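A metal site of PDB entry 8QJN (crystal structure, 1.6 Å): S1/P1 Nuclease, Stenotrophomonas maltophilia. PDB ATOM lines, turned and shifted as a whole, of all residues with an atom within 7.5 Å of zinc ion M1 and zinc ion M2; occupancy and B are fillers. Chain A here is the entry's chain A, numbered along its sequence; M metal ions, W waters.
A ring nitrogen (ND1) of His 62 lies close to the guanidinium group (NH1) of Arg 48 (3.2 Å).
ND1 of His 125 sits at hydrogen-bond distance from O of His 62, 2.7 Å away.
The backbone carbonyl oxygen of His 115 lies close to a ring nitrogen (ND1) of His 6 (3.5 Å).
O of Ala 41 is in hydrogen-bond range of ND1 of His 115, 2.8 Å away.
The side-chain carboxylate (OD1) of Asp 153 lies close to the backbone NH (N) of Trp 1 (3.1 Å).
The indole nitrogen (NE1) of Trp 1 is in hydrogen-bond range of the backbone carbonyl oxygen (O) of Gly 118, 2.8 Å away.
The side-chain carboxylate (OD1) of Asp 45 lies close to the guanidinium group (NH1) of Arg 48, 3.2 Å away.
The nearest printed residue that does not touch zinc ion M1 is His 125 (4.1 Å).
NH1 of Arg 48 touches zinc ion M2, at 3.8 Å.
Of the 25 residues printed, 5 come within 4 Å of zinc ion M2.
Zinc ion M1 is bound by NE2 of His 6, water W2, OD1 of Asp 119, N of Trp 1, O of Trp 1 and water W1.
Zinc ion M2 is bound by water W2 (1.8 Å), OD2 of Asp 119 (2.0 Å), ND1 of His 62 (2.0 Å), NE2 of His 115 (2.1 Å) and OD1 of Asp 45 (2.4 Å).
Zinc ion M2 has five donor atoms within binding distance.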
ATOM      1  N   TRP A   1      32.460 -23.781  11.121  1.00  0.00           N
ATOM      2  CA  TRP A   1      32.377 -25.138  11.677  1.00  0.00           C
ATOM      3  C   TRP A   1      31.462 -26.002  10.808  1.00  0.00           C
ATOM      4  O   TRP A   1      30.593 -25.425  10.080  1.00  0.00           O
ATOM      5  CB  TRP A   1      31.856 -25.129  13.145  1.00  0.00           C
ATOM      6  CG  TRP A   1      32.650 -24.246  14.051  1.00  0.00           C
ATOM      7  CD1 TRP A   1      32.278 -22.999  14.487  1.00  0.00           C
ATOM      8  CD2 TRP A   1      33.932 -24.519  14.648  1.00  0.00           C
ATOM      9  NE1 TRP A   1      33.263 -22.472  15.282  1.00  0.00           N
ATOM     10  CE2 TRP A   1      34.271 -23.400  15.441  1.00  0.00           C
ATOM     11  CE3 TRP A   1      34.793 -25.628  14.656  1.00  0.00           C
ATOM     12  CZ2 TRP A   1      35.442 -23.345  16.191  1.00  0.00           C
ATOM     13  CZ3 TRP A   1      35.980 -25.555  15.361  1.00  0.00           C
ATOM     14  CH2 TRP A   1      36.315 -24.427  16.117  1.00  0.00           C
ATOM     15  N   GLY A   2      31.603 -27.307  10.943  1.00  0.00           N
ATOM     16  CA  GLY A   2      30.564 -28.273  10.536  1.00  0.00           C
ATOM     17  C   GLY A   2      29.409 -28.261  11.496  1.00  0.00           C
ATOM     18  O   GLY A   2      29.440 -27.456  12.460  1.00  0.00           O
ATOM     19  N   ALA A   3      28.417 -29.126  11.278  1.00  0.00           N
ATOM     20  CA  ALA A   3      27.138 -29.081  11.990  1.00  0.00           C
ATOM     21  C   ALA A   3      27.405 -29.241  13.493  1.00  0.00           C
ATOM     22  O   ALA A   3      26.814 -28.494  14.315  1.00  0.00           O
ATOM     23  CB  ALA A   3      26.175 -30.153  11.485  1.00  0.00           C
ATOM     24  N   GLY A   5      30.044 -28.645  15.414  1.00  0.00           N
ATOM     25  CA  GLY A   5      30.637 -27.449  16.032  1.00  0.00           C
ATOM     26  C   GLY A   5      29.571 -26.391  16.265  1.00  0.00           C
ATOM     27  O   GLY A   5      29.559 -25.789  17.375  1.00  0.00           O
ATOM     28  N   HIS A   6      28.717 -26.130  15.265  1.00  0.00           N
ATOM     29  CA  HIS A   6      27.627 -25.139  15.408  1.00  0.00           C
ATOM     30  C   HIS A   6      26.685 -25.533  16.525  1.00  0.00           C
ATOM     31  O   HIS A   6      26.349 -24.620  17.342  1.00  0.00           O
ATOM     32  CB  HIS A   6      26.892 -24.915  14.096  1.00  0.00           C
ATOM     33  CG  HIS A   6      27.747 -24.088  13.207  1.00  0.00           C
ATOM     34  ND1 HIS A   6      27.991 -22.760  13.465  1.00  0.00           N
ATOM     35  CD2 HIS A   6      28.447 -24.410  12.109  1.00  0.00           C
ATOM     36  CE1 HIS A   6      28.792 -22.289  12.523  1.00  0.00           C
ATOM     37  NE2 HIS A   6      29.107 -23.287  11.671  1.00  0.00           N
ATOM     38  N   ALA A  41      21.199 -24.232  14.821  1.00  0.00           N
ATOM     39  CA  ALA A  41      22.567 -23.675  14.719  1.00  0.00           C
ATOM     40  C   ALA A  41      23.166 -23.952  13.351  1.00  0.00           C
ATOM     41  O   ALA A  41      23.851 -23.076  12.816  1.00  0.00           O
ATOM     42  CB  ALA A  41      23.466 -24.158  15.822  1.00  0.00           C
ATOM     43  N   PRO A  42      22.978 -25.139  12.726  1.00  0.00           N
ATOM     44  CA  PRO A  42      23.526 -25.373  11.392  1.00  0.00           C
ATOM     45  C   PRO A  42      22.740 -24.807  10.203  1.00  0.00           C
ATOM     46  O   PRO A  42      23.223 -24.931   9.080  1.00  0.00           O
ATOM     47  CB  PRO A  42      23.542 -26.896  11.278  1.00  0.00           C
ATOM     48  CG  PRO A  42      23.314 -27.388  12.690  1.00  0.00           C
ATOM     49  CD  PRO A  42      22.394 -26.357  13.317  1.00  0.00           C
ATOM     50  N   ALA A  44      22.098 -21.980   8.743  1.00  0.00           N
ATOM     51  CA  ALA A  44      22.623 -21.023   7.741  1.00  0.00           C
ATOM     52  C   ALA A  44      23.441 -21.754   6.662  1.00  0.00           C
ATOM     53  O   ALA A  44      23.526 -21.248   5.522  1.00  0.00           O
ATOM     54  CB  ALA A  44      23.418 -19.943   8.425  1.00  0.00           C
ATOM     55  N   ASP A  45      24.040 -22.902   7.003  1.00  0.00           N
ATOM     56  CA  ASP A  45      24.845 -23.719   6.060  1.00  0.00           C
ATOM     57  C   ASP A  45      23.925 -24.493   5.110  1.00  0.00           C
ATOM     58  O   ASP A  45      24.360 -24.774   4.001  1.00  0.00           O
ATOM     59  CB  ASP A  45      25.804 -24.676   6.783  1.00  0.00           C
ATOM     60  CG  ASP A  45      27.061 -24.004   7.352  1.00  0.00           C
ATOM     61  OD1 ASP A  45      27.337 -22.840   7.009  1.00  0.00           O
ATOM     62  OD2 ASP A  45      27.763 -24.659   8.185  1.00  0.00           O
ATOM     63  N   GLN A  46      22.733 -24.879   5.552  1.00  0.00           N
ATOM     64  CA  GLN A  46      21.813 -25.737   4.770  1.00  0.00           C
ATOM     65  C   GLN A  46      21.077 -24.856   3.744  1.00  0.00           C
ATOM     66  O   GLN A  46      20.669 -25.355   2.717  1.00  0.00           O
ATOM     67  CB  GLN A  46      20.830 -26.468   5.679  1.00  0.00           C
ATOM     68  CG  GLN A  46      21.442 -27.201   6.867  1.00  0.00           C
ATOM     69  CD  GLN A  46      22.842 -27.734   6.710  1.00  0.00           C
ATOM     70  OE1 GLN A  46      23.181 -28.422   5.735  1.00  0.00           O
ATOM     71  NE2 GLN A  46      23.691 -27.465   7.701  1.00  0.00           N
ATOM     72  N   ARG A  48      22.414 -21.801   2.524  1.00  0.00           N
ATOM     73  CA  ARG A  48      23.510 -21.543   1.555  1.00  0.00           C
ATOM     74  C   ARG A  48      23.645 -22.725   0.589  1.00  0.00           C
ATOM     75  O   ARG A  48      23.961 -22.498  -0.610  1.00  0.00           O
ATOM     76  CB  ARG A  48      24.828 -21.325   2.292  1.00  0.00           C
ATOM     77  CG  ARG A  48      25.991 -20.979   1.383  1.00  0.00           C
ATOM     78  CD  ARG A  48      27.318 -21.062   2.120  1.00  0.00           C
ATOM     79  NE  ARG A  48      27.534 -22.396   2.662  1.00  0.00           N
ATOM     80  CZ  ARG A  48      28.241 -22.671   3.761  1.00  0.00           C
ATOM     81  NH1 ARG A  48      28.813 -21.701   4.444  1.00  0.00           N
ATOM     82  NH2 ARG A  48      28.358 -23.923   4.172  1.00  0.00           N
ATOM     83  N   ALA A  59      25.934 -16.296   1.434  1.00  0.00           N
ATOM     84  CA  ALA A  59      27.071 -17.240   1.368  1.00  0.00           C
ATOM     85  C   ALA A  59      28.352 -16.552   1.873  1.00  0.00           C
ATOM     86  O   ALA A  59      29.113 -17.232   2.581  1.00  0.00           O
ATOM     87  CB  ALA A  59      27.254 -17.746  -0.048  1.00  0.00           C
ATOM     88  N   TRP A  61      28.597 -14.325   4.104  1.00  0.00           N
ATOM     89  CA  TRP A  61      28.416 -13.855   5.492  1.00  0.00           C
ATOM     90  C   TRP A  61      29.152 -14.801   6.456  1.00  0.00           C
ATOM     91  O   TRP A  61      29.271 -14.455   7.621  1.00  0.00           O
ATOM     92  CB  TRP A  61      26.929 -13.815   5.837  1.00  0.00           C
ATOM     93  CG  TRP A  61      26.112 -12.821   5.077  1.00  0.00           C
ATOM     94  CD1 TRP A  61      26.488 -11.941   4.081  1.00  0.00           C
ATOM     95  CD2 TRP A  61      24.711 -12.614   5.301  1.00  0.00           C
ATOM     96  NE1 TRP A  61      25.389 -11.223   3.660  1.00  0.00           N
ATOM     97  CE2 TRP A  61      24.303 -11.620   4.378  1.00  0.00           C
ATOM     98  CE3 TRP A  61      23.777 -13.157   6.187  1.00  0.00           C
ATOM     99  CZ2 TRP A  61      23.001 -11.130   4.380  1.00  0.00           C
ATOM    100  CZ3 TRP A  61      22.479 -12.716   6.129  1.00  0.00           C
ATOM    101  CH2 TRP A  61      22.101 -11.740   5.210  1.00  0.00           C
ATOM    102  N   HIS A  62      29.587 -15.992   5.991  1.00  0.00           N
ATOM    103  CA  HIS A  62      30.168 -17.006   6.895  1.00  0.00           C
ATOM    104  C   HIS A  62      31.638 -16.700   7.210  1.00  0.00           C
ATOM    105  O   HIS A  62      32.209 -17.392   8.045  1.00  0.00           O
ATOM    106  CB  HIS A  62      29.970 -18.398   6.341  1.00  0.00           C
ATOM    107  CG  HIS A  62      28.556 -18.798   6.249  1.00  0.00           C
ATOM    108  ND1 HIS A  62      28.047 -19.900   6.913  1.00  0.00           N
ATOM    109  CD2 HIS A  62      27.552 -18.268   5.514  1.00  0.00           C
ATOM    110  CE1 HIS A  62      26.762 -19.982   6.633  1.00  0.00           C
ATOM    111  NE2 HIS A  62      26.425 -18.993   5.784  1.00  0.00           N
ATOM    112  N   TYR A  63      32.266 -15.761   6.542  1.00  0.00           N
ATOM    113  CA  TYR A  63      33.731 -15.578   6.710  1.00  0.00           C
ATOM    114  C   TYR A  63      34.154 -14.148   6.431  1.00  0.00           C
ATOM    115  O   TYR A  63      33.361 -13.289   6.026  1.00  0.00           O
ATOM    116  CB  TYR A  63      34.485 -16.572   5.820  1.00  0.00           C
ATOM    117  CG  TYR A  63      34.113 -16.498   4.382  1.00  0.00           C
ATOM    118  CD1 TYR A  63      34.731 -15.574   3.540  1.00  0.00           C
ATOM    119  CD2 TYR A  63      33.121 -17.308   3.851  1.00  0.00           C
ATOM    120  CE1 TYR A  63      34.373 -15.469   2.199  1.00  0.00           C
ATOM    121  CE2 TYR A  63      32.752 -17.210   2.521  1.00  0.00           C
ATOM    122  CZ  TYR A  63      33.376 -16.292   1.702  1.00  0.00           C
ATOM    123  OH  TYR A  63      33.030 -16.191   0.369  1.00  0.00           O
ATOM    124  N   ILE A  85      31.328 -11.723   7.488  1.00  0.00           N
ATOM    125  CA  ILE A  85      30.737 -12.140   8.792  1.00  0.00           C
ATOM    126  C   ILE A  85      30.733 -10.985   9.775  1.00  0.00           C
ATOM    127  O   ILE A  85      29.813 -10.980  10.637  1.00  0.00           O
ATOM    128  CB  ILE A  85      31.476 -13.365   9.355  1.00  0.00           C
ATOM    129  CG1 ILE A  85      30.692 -13.994  10.515  1.00  0.00           C
ATOM    130  CG2 ILE A  85      32.908 -13.020   9.742  1.00  0.00           C
ATOM    131  CD1 ILE A  85      31.143 -15.400  10.786  1.00  0.00           C
ATOM    132  N   HIS A 115      24.559 -19.013  14.328  1.00  0.00           N
ATOM    133  CA  HIS A 115      25.481 -19.650  13.369  1.00  0.00           C
ATOM    134  C   HIS A 115      26.740 -18.763  13.295  1.00  0.00           C
ATOM    135  O   HIS A 115      27.852 -19.307  13.368  1.00  0.00           O
ATOM    136  CB  HIS A 115      24.842 -19.798  11.981  1.00  0.00           C
ATOM    137  CG  HIS A 115      25.701 -20.600  11.060  1.00  0.00           C
ATOM    138  ND1 HIS A 115      25.597 -21.970  10.970  1.00  0.00           N
ATOM    139  CD2 HIS A 115      26.694 -20.244  10.219  1.00  0.00           C
ATOM    140  CE1 HIS A 115      26.461 -22.429  10.096  1.00  0.00           C
ATOM    141  NE2 HIS A 115      27.166 -21.407   9.620  1.00  0.00           N
ATOM    142  N   LEU A 116      26.560 -17.465  13.033  1.00  0.00           N
ATOM    143  CA  LEU A 116      27.728 -16.596  12.753  1.00  0.00           C
ATOM    144  C   LEU A 116      28.600 -16.423  14.004  1.00  0.00           C
ATOM    145  O   LEU A 116      29.790 -16.248  13.847  1.00  0.00           O
ATOM    146  CB  LEU A 116      27.255 -15.268  12.170  1.00  0.00           C
ATOM    147  CG  LEU A 116      26.523 -15.378  10.850  1.00  0.00           C
ATOM    148  CD1 LEU A 116      26.184 -13.989  10.373  1.00  0.00           C
ATOM    149  CD2 LEU A 116      27.317 -16.154   9.802  1.00  0.00           C
ATOM    150  N   GLY A 118      29.287 -18.774  16.028  1.00  0.00           N
ATOM    151  CA  GLY A 118      30.123 -19.968  15.780  1.00  0.00           C
ATOM    152  C   GLY A 118      31.216 -19.660  14.746  1.00  0.00           C
ATOM    153  O   GLY A 118      32.419 -19.849  15.019  1.00  0.00           O
ATOM    154  N   ASP A 119      30.819 -19.271  13.535  1.00  0.00           N
ATOM    155  CA  ASP A 119      31.748 -19.209  12.386  1.00  0.00           C
ATOM    156  C   ASP A 119      32.822 -18.154  12.655  1.00  0.00           C
ATOM    157  O   ASP A 119      33.998 -18.372  12.249  1.00  0.00           O
ATOM    158  CB  ASP A 119      31.055 -18.965  11.057  1.00  0.00           C
ATOM    159  CG  ASP A 119      30.614 -20.206  10.331  1.00  0.00           C
ATOM    160  OD1 ASP A 119      30.980 -21.293  10.802  1.00  0.00           O
ATOM    161  OD2 ASP A 119      29.900 -20.077   9.249  1.00  0.00           O
ATOM    162  N   ILE A 120      32.478 -17.054  13.335  1.00  0.00           N
ATOM    163  CA  ILE A 120      33.474 -15.985  13.576  1.00  0.00           C
ATOM    164  C   ILE A 120      34.532 -16.419  14.604  1.00  0.00           C
ATOM    165  O   ILE A 120      35.537 -15.705  14.731  1.00  0.00           O
ATOM    166  CB  ILE A 120      32.766 -14.670  13.938  1.00  0.00           C
ATOM    167  CG1 ILE A 120      33.599 -13.449  13.577  1.00  0.00           C
ATOM    168  CG2 ILE A 120      32.352 -14.697  15.401  1.00  0.00           C
ATOM    169  CD1 ILE A 120      32.807 -12.166  13.652  1.00  0.00           C
ATOM    170  N   GLN A 122      35.801 -19.642  14.277  1.00  0.00           N
ATOM    171  CA  GLN A 122      36.559 -20.693  13.539  1.00  0.00           C
ATOM    172  C   GLN A 122      37.723 -19.995  12.832  1.00  0.00           C
ATOM    173  O   GLN A 122      37.516 -19.205  11.916  1.00  0.00           O
ATOM    174  CB  GLN A 122      35.676 -21.446  12.543  1.00  0.00           C
ATOM    175  CG  GLN A 122      36.094 -22.907  12.313  1.00  0.00           C
ATOM    176  CD  GLN A 122      37.327 -23.096  11.470  1.00  0.00           C
ATOM    177  OE1 GLN A 122      38.412 -22.650  11.809  1.00  0.00           O
ATOM    178  NE2 GLN A 122      37.178 -23.820  10.363  1.00  0.00           N
ATOM    179  N   HIS A 125      37.803 -19.419   9.195  1.00  0.00           N
ATOM    180  CA  HIS A 125      36.764 -18.507   8.660  1.00  0.00           C
ATOM    181  C   HIS A 125      37.253 -17.042   8.724  1.00  0.00           C
ATOM    182  O   HIS A 125      36.477 -16.174   8.324  1.00  0.00           O
ATOM    183  CB  HIS A 125      35.440 -18.711   9.399  1.00  0.00           C
ATOM    184  CG  HIS A 125      34.665 -19.879   8.938  1.00  0.00           C
ATOM    185  ND1 HIS A 125      33.428 -19.746   8.399  1.00  0.00           N
ATOM    186  CD2 HIS A 125      34.973 -21.197   8.828  1.00  0.00           C
ATOM    187  CE1 HIS A 125      32.989 -20.919   7.994  1.00  0.00           C
ATOM    188  NE2 HIS A 125      33.887 -21.838   8.285  1.00  0.00           N
ATOM    189  N   HIS A 149      40.925 -26.211   5.890  1.00  0.00           N
ATOM    190  CA  HIS A 149      39.599 -25.675   6.254  1.00  0.00           C
ATOM    191  C   HIS A 149      38.728 -26.750   6.912  1.00  0.00           C
ATOM    192  O   HIS A 149      38.207 -26.481   8.060  1.00  0.00           O
ATOM    193  CB  HIS A 149      38.886 -25.030   5.080  1.00  0.00           C
ATOM    194  CG  HIS A 149      37.716 -24.260   5.563  1.00  0.00           C
ATOM    195  ND1 HIS A 149      37.791 -22.910   5.746  1.00  0.00           N
ATOM    196  CD2 HIS A 149      36.464 -24.627   5.914  1.00  0.00           C
ATOM    197  CE1 HIS A 149      36.637 -22.476   6.217  1.00  0.00           C
ATOM    198  NE2 HIS A 149      35.782 -23.488   6.295  1.00  0.00           N
ATOM    199  N   ASP A 153      37.102 -27.142  10.606  1.00  0.00           N
ATOM    200  CA  ASP A 153      35.617 -27.184  10.724  1.00  0.00           C
ATOM    201  C   ASP A 153      35.151 -28.465  11.431  1.00  0.00           C
ATOM    202  O   ASP A 153      34.233 -28.345  12.226  1.00  0.00           O
ATOM    203  CB  ASP A 153      34.898 -27.084   9.386  1.00  0.00           C
ATOM    204  CG  ASP A 153      34.620 -25.702   8.868  1.00  0.00           C
ATOM    205  OD1 ASP A 153      34.939 -24.726   9.557  1.00  0.00           O
ATOM    206  OD2 ASP A 153      34.042 -25.626   7.783  1.00  0.00           O
HETATM  207 ZN    ZN M   1      30.550 -23.239  10.255  1.00  0.00          ZN
HETATM  208 ZN    ZN M   2      28.693 -21.297   8.210  1.00  0.00          ZN
HETATM  209 ZN    ZN M   3      33.989 -23.639   7.245  1.00  0.00          ZN
HETATM  210  O   HOH W   1      31.648 -24.041   8.166  1.00  0.00           O
HETATM  211  O   HOH W   2      29.908 -22.626   8.422  1.00  0.00           O
